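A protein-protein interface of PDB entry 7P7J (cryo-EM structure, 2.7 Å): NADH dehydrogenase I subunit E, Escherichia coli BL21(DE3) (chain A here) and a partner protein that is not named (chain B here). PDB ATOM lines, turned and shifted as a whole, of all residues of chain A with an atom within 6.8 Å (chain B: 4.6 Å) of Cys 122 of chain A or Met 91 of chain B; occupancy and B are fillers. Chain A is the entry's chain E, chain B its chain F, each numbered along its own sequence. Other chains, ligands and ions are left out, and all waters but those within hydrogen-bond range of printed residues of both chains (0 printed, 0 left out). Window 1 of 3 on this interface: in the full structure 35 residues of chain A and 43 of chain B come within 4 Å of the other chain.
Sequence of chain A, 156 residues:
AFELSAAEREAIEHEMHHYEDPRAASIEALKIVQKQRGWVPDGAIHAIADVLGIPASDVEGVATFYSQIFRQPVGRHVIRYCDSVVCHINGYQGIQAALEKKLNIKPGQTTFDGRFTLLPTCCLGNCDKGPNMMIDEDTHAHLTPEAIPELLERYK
NH2 of Arg 130 of chain B lies within hydrogen-bond range of O of Cys 123 of chain A (2.5 Å).
The guanidinium group (NH2) of Arg 80 of chain A is in salt-bridge range of the side-chain carboxylate (OE2) of Glu 132 of chain B (2.5 Å).
The side-chain carboxylate of Asp 83 of chain A lies within salt-bridge range of the guanidinium group of Arg 345 of chain B.
O of Thr 121 of chain A is in hydrogen-bond range of NH2 of Arg 345 of chain B, 3.0 Å away.
The backbone NH of Cys 122 of chain A sits close to the guanidinium group of Arg 345 of chain B.
N of Gly 125 of chain A lies close to NH1 of Arg 130 of chain B (3.5 Å).
The side-chain carboxylate of Glu 132 of chain B lies within salt-bridge range of the guanidinium group of Arg 130 of chain B, 2.5 Å away.
The side-chain amide oxygen of Gln 68 of chain A sits close to the guanidinium group of Arg 80 of chain A, 3.2 Å away.
The backbone NH (N) of Thr 121 of chain A lies within hydrogen-bond range of the backbone carbonyl oxygen (O) of Tyr 81 of chain A (2.9 Å).
SG of Cys 82 of chain A lies close to N of Ser 84 of chain A, 3.6 Å away.
The side-chain sulfur (SG) of Cys 82 of chain A lies close to the backbone carbonyl oxygen (O) of Cys 122 of chain A (3.5 Å).
The backbone NH (N) of Asp 83 of chain A sits at hydrogen-bond distance from the backbone carbonyl oxygen (O) of Thr 121 of chain A (3.3 Å).
Among the printed residues, pairs that only touch across the chains: Leu 124 of chain A with Arg 130 of chain B, Cys 122 of chain A with Met 91 of chain B, Cys 123 of chain A with Pro 93 of chain B, Ser 67 of chain A with Arg 174 of chain B, Cys 122 of chain A with Arg 130 of chain B and Ser 84 of chain A with Phe 342 of chain B.
Met 91 of chain B touches just one residue of chain A: Cys 122 (3.5 Å).
Of the printed residues of chain B, Arg 80 of chain A touches Glu 132.
Printed residues of chain A within 4 Å of Arg 130 of chain B: Cys 122 (3.9 Å), Cys 123 (2.5 Å), Leu 124 (3.4 Å) and Gly 125 (3.5 Å).
Of the printed residues of chain A, Arg 174 of chain B touches Ser 67.
Of the printed residues of chain A, Glu 132 of chain B touches Arg 80 (2.5 Å).
Of the 13 printed residues of chain A, 9 touch a printed residue of chain B.
Printed residues of chain B that touch a printed residue of chain A: Met 91, Pro 93, Arg 130, Glu 132, Arg 174, Phe 342 and Arg 345.
Hydrophobic or aromatic side chains of chain B within 4 Å of the printed part of chain A: Met 91, Pro 93 and Phe 342.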
ATOM      1  N   SER A  67     -27.732  26.460 -27.133  1.00  0.00           N
ATOM      2  CA  SER A  67     -27.941  27.866 -26.811  1.00  0.00           C
ATOM      3  C   SER A  67     -26.673  28.691 -26.976  1.00  0.00           C
ATOM      4  O   SER A  67     -26.754  29.888 -27.269  1.00  0.00           O
ATOM      5  CB  SER A  67     -28.477  27.995 -25.388  1.00  0.00           C
ATOM      6  OG  SER A  67     -27.719  27.206 -24.489  1.00  0.00           O
ATOM      7  N   GLN A  68     -25.503  28.084 -26.800  1.00  0.00           N
ATOM      8  CA  GLN A  68     -24.247  28.817 -26.839  1.00  0.00           C
ATOM      9  C   GLN A  68     -23.639  28.886 -28.230  1.00  0.00           C
ATOM     10  O   GLN A  68     -22.530  29.406 -28.383  1.00  0.00           O
ATOM     11  CB  GLN A  68     -23.243  28.202 -25.864  1.00  0.00           C
ATOM     12  CG  GLN A  68     -23.762  28.075 -24.443  1.00  0.00           C
ATOM     13  CD  GLN A  68     -24.241  29.394 -23.870  1.00  0.00           C
ATOM     14  OE1 GLN A  68     -23.623  30.439 -24.078  1.00  0.00           O
ATOM     15  NE2 GLN A  68     -25.349  29.352 -23.141  1.00  0.00           N
ATOM     16  N   ARG A  80     -23.749  36.989 -19.580  1.00  0.00           N
ATOM     17  CA  ARG A  80     -24.612  35.827 -19.383  1.00  0.00           C
ATOM     18  C   ARG A  80     -24.950  35.757 -17.899  1.00  0.00           C
ATOM     19  O   ARG A  80     -24.158  35.247 -17.101  1.00  0.00           O
ATOM     20  CB  ARG A  80     -23.936  34.549 -19.861  1.00  0.00           C
ATOM     21  CG  ARG A  80     -24.212  34.216 -21.313  1.00  0.00           C
ATOM     22  CD  ARG A  80     -23.322  33.087 -21.777  1.00  0.00           C
ATOM     23  NE  ARG A  80     -23.730  31.831 -21.163  1.00  0.00           N
ATOM     24  CZ  ARG A  80     -22.957  30.761 -21.047  1.00  0.00           C
ATOM     25  NH1 ARG A  80     -21.706  30.762 -21.475  1.00  0.00           N
ATOM     26  NH2 ARG A  80     -23.455  29.663 -20.488  1.00  0.00           N
ATOM     27  N   TYR A  81     -26.121  36.261 -17.528  1.00  0.00           N
ATOM     28  CA  TYR A  81     -26.511  36.274 -16.126  1.00  0.00           C
ATOM     29  C   TYR A  81     -27.340  35.038 -15.812  1.00  0.00           C
ATOM     30  O   TYR A  81     -28.211  34.644 -16.591  1.00  0.00           O
ATOM     31  CB  TYR A  81     -27.278  37.552 -15.772  1.00  0.00           C
ATOM     32  CG  TYR A  81     -28.623  37.718 -16.444  1.00  0.00           C
ATOM     33  CD1 TYR A  81     -28.730  38.334 -17.682  1.00  0.00           C
ATOM     34  CD2 TYR A  81     -29.792  37.298 -15.817  1.00  0.00           C
ATOM     35  CE1 TYR A  81     -29.955  38.495 -18.292  1.00  0.00           C
ATOM     36  CE2 TYR A  81     -31.018  37.453 -16.421  1.00  0.00           C
ATOM     37  CZ  TYR A  81     -31.095  38.055 -17.657  1.00  0.00           C
ATOM     38  OH  TYR A  81     -32.321  38.214 -18.257  1.00  0.00           O
ATOM     39  N   CYS A  82     -27.049  34.415 -14.675  1.00  0.00           N
ATOM     40  CA  CYS A  82     -27.711  33.173 -14.300  1.00  0.00           C
ATOM     41  C   CYS A  82     -29.098  33.475 -13.751  1.00  0.00           C
ATOM     42  O   CYS A  82     -29.234  34.205 -12.764  1.00  0.00           O
ATOM     43  CB  CYS A  82     -26.876  32.418 -13.272  1.00  0.00           C
ATOM     44  SG  CYS A  82     -27.587  30.846 -12.771  1.00  0.00           S
ATOM     45  N   ASP A  83     -30.126  32.916 -14.387  1.00  0.00           N
ATOM     46  CA  ASP A  83     -31.503  33.106 -13.954  1.00  0.00           C
ATOM     47  C   ASP A  83     -32.068  31.899 -13.215  1.00  0.00           C
ATOM     48  O   ASP A  83     -33.278  31.843 -12.979  1.00  0.00           O
ATOM     49  CB  ASP A  83     -32.396  33.473 -15.150  1.00  0.00           C
ATOM     50  CG  ASP A  83     -32.397  32.426 -16.264  1.00  0.00           C
ATOM     51  OD1 ASP A  83     -31.919  31.288 -16.083  1.00  0.00           O
ATOM     52  OD2 ASP A  83     -32.908  32.756 -17.353  1.00  0.00           O
ATOM     53  N   SER A  84     -31.227  30.939 -12.845  1.00  0.00           N
ATOM     54  CA  SER A  84     -31.705  29.687 -12.275  1.00  0.00           C
ATOM     55  C   SER A  84     -32.089  29.890 -10.810  1.00  0.00           C
ATOM     56  O   SER A  84     -32.098  31.008 -10.288  1.00  0.00           O
ATOM     57  CB  SER A  84     -30.663  28.591 -12.462  1.00  0.00           C
ATOM     58  OG  SER A  84     -30.513  28.261 -13.830  1.00  0.00           O
ATOM     59  N   PRO A 120     -29.879  35.938 -20.597  1.00  0.00           N
ATOM     60  CA  PRO A 120     -30.141  35.015 -19.488  1.00  0.00           C
ATOM     61  C   PRO A 120     -29.592  33.641 -19.830  1.00  0.00           C
ATOM     62  O   PRO A 120     -29.815  33.124 -20.926  1.00  0.00           O
ATOM     63  CB  PRO A 120     -31.670  35.009 -19.382  1.00  0.00           C
ATOM     64  CG  PRO A 120     -32.144  35.410 -20.735  1.00  0.00           C
ATOM     65  CD  PRO A 120     -31.116  36.360 -21.276  1.00  0.00           C
ATOM     66  N   THR A 121     -28.862  33.054 -18.894  1.00  0.00           N
ATOM     67  CA  THR A 121     -28.211  31.779 -19.121  1.00  0.00           C
ATOM     68  C   THR A 121     -28.648  30.775 -18.065  1.00  0.00           C
ATOM     69  O   THR A 121     -29.262  31.118 -17.052  1.00  0.00           O
ATOM     70  CB  THR A 121     -26.682  31.924 -19.116  1.00  0.00           C
ATOM     71  OG1 THR A 121     -26.084  30.725 -19.622  1.00  0.00           O
ATOM     72  CG2 THR A 121     -26.170  32.178 -17.710  1.00  0.00           C
ATOM     73  N   CYS A 122     -28.302  29.519 -18.319  1.00  0.00           N
ATOM     74  CA  CYS A 122     -28.600  28.417 -17.421  1.00  0.00           C
ATOM     75  C   CYS A 122     -27.735  28.501 -16.163  1.00  0.00           C
ATOM     76  O   CYS A 122     -26.957  29.438 -15.965  1.00  0.00           O
ATOM     77  CB  CYS A 122     -28.386  27.101 -18.159  1.00  0.00           C
ATOM     78  SG  CYS A 122     -26.888  27.135 -19.171  1.00  0.00           S
ATOM     79  N   CYS A 123     -27.884  27.505 -15.294  1.00  0.00           N
ATOM     80  CA  CYS A 123     -27.095  27.455 -14.070  1.00  0.00           C
ATOM     81  C   CYS A 123     -25.624  27.246 -14.400  1.00  0.00           C
ATOM     82  O   CYS A 123     -25.271  26.355 -15.175  1.00  0.00           O
ATOM     83  CB  CYS A 123     -27.594  26.340 -13.159  1.00  0.00           C
ATOM     84  SG  CYS A 123     -26.421  25.883 -11.871  1.00  0.00           S
ATOM     85  N   LEU A 124     -24.767  28.072 -13.807  1.00  0.00           N
ATOM     86  CA  LEU A 124     -23.346  28.077 -14.119  1.00  0.00           C
ATOM     87  C   LEU A 124     -22.540  27.119 -13.256  1.00  0.00           C
ATOM     88  O   LEU A 124     -21.312  27.084 -13.380  1.00  0.00           O
ATOM     89  CB  LEU A 124     -22.782  29.493 -13.976  1.00  0.00           C
ATOM     90  CG  LEU A 124     -23.374  30.550 -14.908  1.00  0.00           C
ATOM     91  CD1 LEU A 124     -22.790  31.914 -14.602  1.00  0.00           C
ATOM     92  CD2 LEU A 124     -23.133  30.183 -16.360  1.00  0.00           C
ATOM     93  N   GLY A 125     -23.189  26.346 -12.390  1.00  0.00           N
ATOM     94  CA  GLY A 125     -22.465  25.438 -11.522  1.00  0.00           C
ATOM     95  C   GLY A 125     -21.679  26.127 -10.433  1.00  0.00           C
ATOM     96  O   GLY A 125     -20.686  25.577  -9.949  1.00  0.00           O
ATOM     97  N   ASP B  89     -21.079  17.119 -17.389  1.00  0.00           N
ATOM     98  CA  ASP B  89     -21.948  18.217 -17.794  1.00  0.00           C
ATOM     99  C   ASP B  89     -22.362  19.064 -16.598  1.00  0.00           C
ATOM    100  O   ASP B  89     -22.190  20.287 -16.610  1.00  0.00           O
ATOM    101  CB  ASP B  89     -23.175  17.664 -18.519  1.00  0.00           C
ATOM    102  CG  ASP B  89     -23.669  18.583 -19.614  1.00  0.00           C
ATOM    103  OD1 ASP B  89     -22.909  19.481 -20.028  1.00  0.00           O
ATOM    104  OD2 ASP B  89     -24.819  18.412 -20.063  1.00  0.00           O
ATOM    105  N   GLU B  90     -22.877  18.415 -15.546  1.00  0.00           N
ATOM    106  CA  GLU B  90     -23.308  19.062 -14.298  1.00  0.00           C
ATOM    107  C   GLU B  90     -24.272  20.217 -14.559  1.00  0.00           C
ATOM    108  O   GLU B  90     -24.167  21.293 -13.967  1.00  0.00           O
ATOM    109  CB  GLU B  90     -22.113  19.528 -13.469  1.00  0.00           C
ATOM    110  CG  GLU B  90     -22.330  19.359 -11.977  1.00  0.00           C
ATOM    111  CD  GLU B  90     -21.334  20.129 -11.145  1.00  0.00           C
ATOM    112  OE1 GLU B  90     -20.796  21.141 -11.639  1.00  0.00           O
ATOM    113  OE2 GLU B  90     -21.086  19.718  -9.995  1.00  0.00           O
ATOM    114  N   MET B  91     -25.213  19.990 -15.467  1.00  0.00           N
ATOM    115  CA  MET B  91     -26.139  21.030 -15.885  1.00  0.00           C
ATOM    116  C   MET B  91     -27.330  21.189 -14.953  1.00  0.00           C
ATOM    117  O   MET B  91     -28.111  22.129 -15.137  1.00  0.00           O
ATOM    118  CB  MET B  91     -26.627  20.736 -17.307  1.00  0.00           C
ATOM    119  CG  MET B  91     -25.696  21.172 -18.439  1.00  0.00           C
ATOM    120  SD  MET B  91     -25.146  22.892 -18.507  1.00  0.00           S
ATOM    121  CE  MET B  91     -26.627  23.793 -18.047  1.00  0.00           C
ATOM    122  N   GLU B  92     -27.491  20.306 -13.976  1.00  0.00           N
ATOM    123  CA  GLU B  92     -28.582  20.440 -13.019  1.00  0.00           C
ATOM    124  C   GLU B  92     -28.341  21.651 -12.125  1.00  0.00           C
ATOM    125  O   GLU B  92     -27.229  21.818 -11.610  1.00  0.00           O
ATOM    126  CB  GLU B  92     -28.706  19.174 -12.176  1.00  0.00           C
ATOM    127  CG  GLU B  92     -29.744  19.255 -11.066  1.00  0.00           C
ATOM    128  CD  GLU B  92     -31.070  18.631 -11.453  1.00  0.00           C
ATOM    129  OE1 GLU B  92     -31.640  19.033 -12.486  1.00  0.00           O
ATOM    130  OE2 GLU B  92     -31.541  17.733 -10.723  1.00  0.00           O
ATOM    131  N   PRO B  93     -29.327  22.529 -11.949  1.00  0.00           N
ATOM    132  CA  PRO B  93     -29.165  23.644 -11.010  1.00  0.00           C
ATOM    133  C   PRO B  93     -29.013  23.154  -9.579  1.00  0.00           C
ATOM    134  O   PRO B  93     -29.587  22.140  -9.178  1.00  0.00           O
ATOM    135  CB  PRO B  93     -30.454  24.451 -11.191  1.00  0.00           C
ATOM    136  CG  PRO B  93     -30.921  24.103 -12.553  1.00  0.00           C
ATOM    137  CD  PRO B  93     -30.550  22.665 -12.756  1.00  0.00           C
ATOM    138  N   ARG B 130     -19.176  20.489 -19.762  1.00  0.00           N
ATOM    139  CA  ARG B 130     -19.920  21.654 -20.209  1.00  0.00           C
ATOM    140  C   ARG B 130     -18.963  22.758 -20.653  1.00  0.00           C
ATOM    141  O   ARG B 130     -17.796  22.806 -20.259  1.00  0.00           O
ATOM    142  CB  ARG B 130     -20.847  22.162 -19.107  1.00  0.00           C
ATOM    143  CG  ARG B 130     -20.137  22.867 -17.977  1.00  0.00           C
ATOM    144  CD  ARG B 130     -21.111  23.310 -16.909  1.00  0.00           C
ATOM    145  NE  ARG B 130     -22.038  24.329 -17.381  1.00  0.00           N
ATOM    146  CZ  ARG B 130     -22.974  24.885 -16.628  1.00  0.00           C
ATOM    147  NH1 ARG B 130     -23.144  24.533 -15.365  1.00  0.00           N
ATOM    148  NH2 ARG B 130     -23.761  25.817 -17.154  1.00  0.00           N
ATOM    149  N   GLU B 132     -19.007  25.900 -19.971  1.00  0.00           N
ATOM    150  CA  GLU B 132     -18.778  26.958 -19.000  1.00  0.00           C
ATOM    151  C   GLU B 132     -17.620  26.664 -18.060  1.00  0.00           C
ATOM    152  O   GLU B 132     -17.142  27.580 -17.382  1.00  0.00           O
ATOM    153  CB  GLU B 132     -20.043  27.197 -18.173  1.00  0.00           C
ATOM    154  CG  GLU B 132     -21.181  27.823 -18.950  1.00  0.00           C
ATOM    155  CD  GLU B 132     -22.011  26.805 -19.709  1.00  0.00           C
ATOM    156  OE1 GLU B 132     -21.823  25.592 -19.480  1.00  0.00           O
ATOM    157  OE2 GLU B 132     -22.851  27.216 -20.536  1.00  0.00           O
ATOM    158  N   ARG B 174     -26.352  23.049 -23.069  1.00  0.00           N
ATOM    159  CA  ARG B 174     -27.739  22.611 -23.027  1.00  0.00           C
ATOM    160  C   ARG B 174     -27.901  21.627 -21.877  1.00  0.00           C
ATOM    161  O   ARG B 174     -27.038  20.774 -21.657  1.00  0.00           O
ATOM    162  CB  ARG B 174     -28.158  21.980 -24.359  1.00  0.00           C
ATOM    163  CG  ARG B 174     -29.643  21.726 -24.500  1.00  0.00           C
ATOM    164  CD  ARG B 174     -30.457  22.997 -24.345  1.00  0.00           C
ATOM    165  NE  ARG B 174     -30.537  23.786 -25.568  1.00  0.00           N
ATOM    166  CZ  ARG B 174     -31.269  24.885 -25.699  1.00  0.00           C
ATOM    167  NH1 ARG B 174     -31.994  25.354 -24.697  1.00  0.00           N
ATOM    168  NH2 ARG B 174     -31.278  25.525 -26.863  1.00  0.00           N
ATOM    169  N   TYR B 175     -29.003  21.761 -21.135  1.00  0.00           N
ATOM    170  CA  TYR B 175     -29.190  20.963 -19.928  1.00  0.00           C
ATOM    171  C   TYR B 175     -29.502  19.507 -20.244  1.00  0.00           C
ATOM    172  O   TYR B 175     -29.115  18.615 -19.481  1.00  0.00           O
ATOM    173  CB  TYR B 175     -30.299  21.571 -19.069  1.00  0.00           C
ATOM    174  CG  TYR B 175     -30.855  20.654 -18.001  1.00  0.00           C
ATOM    175  CD1 TYR B 175     -30.093  20.288 -16.904  1.00  0.00           C
ATOM    176  CD2 TYR B 175     -32.148  20.162 -18.090  1.00  0.00           C
ATOM    177  CE1 TYR B 175     -30.596  19.454 -15.931  1.00  0.00           C
ATOM    178  CE2 TYR B 175     -32.659  19.331 -17.118  1.00  0.00           C
ATOM    179  CZ  TYR B 175     -31.879  18.979 -16.042  1.00  0.00           C
ATOM    180  OH  TYR B 175     -32.385  18.147 -15.072  1.00  0.00           O
ATOM    181  N   PHE B 342     -37.144  27.293 -16.331  1.00  0.00           N
ATOM    182  CA  PHE B 342     -35.914  26.586 -16.674  1.00  0.00           C
ATOM    183  C   PHE B 342     -36.216  25.247 -17.335  1.00  0.00           C
ATOM    184  O   PHE B 342     -35.672  24.930 -18.395  1.00  0.00           O
ATOM    185  CB  PHE B 342     -35.053  26.379 -15.429  1.00  0.00           C
ATOM    186  CG  PHE B 342     -33.863  25.489 -15.661  1.00  0.00           C
ATOM    187  CD1 PHE B 342     -32.722  25.986 -16.264  1.00  0.00           C
ATOM    188  CD2 PHE B 342     -33.886  24.155 -15.279  1.00  0.00           C
ATOM    189  CE1 PHE B 342     -31.629  25.174 -16.482  1.00  0.00           C
ATOM    190  CE2 PHE B 342     -32.800  23.340 -15.506  1.00  0.00           C
ATOM    191  CZ  PHE B 342     -31.670  23.851 -16.104  1.00  0.00           C
ATOM    192  N   ARG B 345     -37.692  25.702 -20.863  1.00  0.00           N
ATOM    193  CA  ARG B 345     -36.754  26.158 -21.877  1.00  0.00           C
ATOM    194  C   ARG B 345     -35.623  25.170 -22.117  1.00  0.00           C
ATOM    195  O   ARG B 345     -34.908  25.302 -23.115  1.00  0.00           O
ATOM    196  CB  ARG B 345     -36.180  27.523 -21.496  1.00  0.00           C
ATOM    197  CG  ARG B 345     -35.016  27.463 -20.540  1.00  0.00           C
ATOM    198  CD  ARG B 345     -34.468  28.847 -20.264  1.00  0.00           C
ATOM    199  NE  ARG B 345     -33.372  28.802 -19.305  1.00  0.00           N
ATOM    200  CZ  ARG B 345     -32.731  29.869 -18.852  1.00  0.00           C
ATOM    201  NH1 ARG B 345     -33.050  31.088 -19.253  1.00  0.00           N
ATOM    202  NH2 ARG B 345     -31.747  29.710 -17.974  1.00  0.00           N
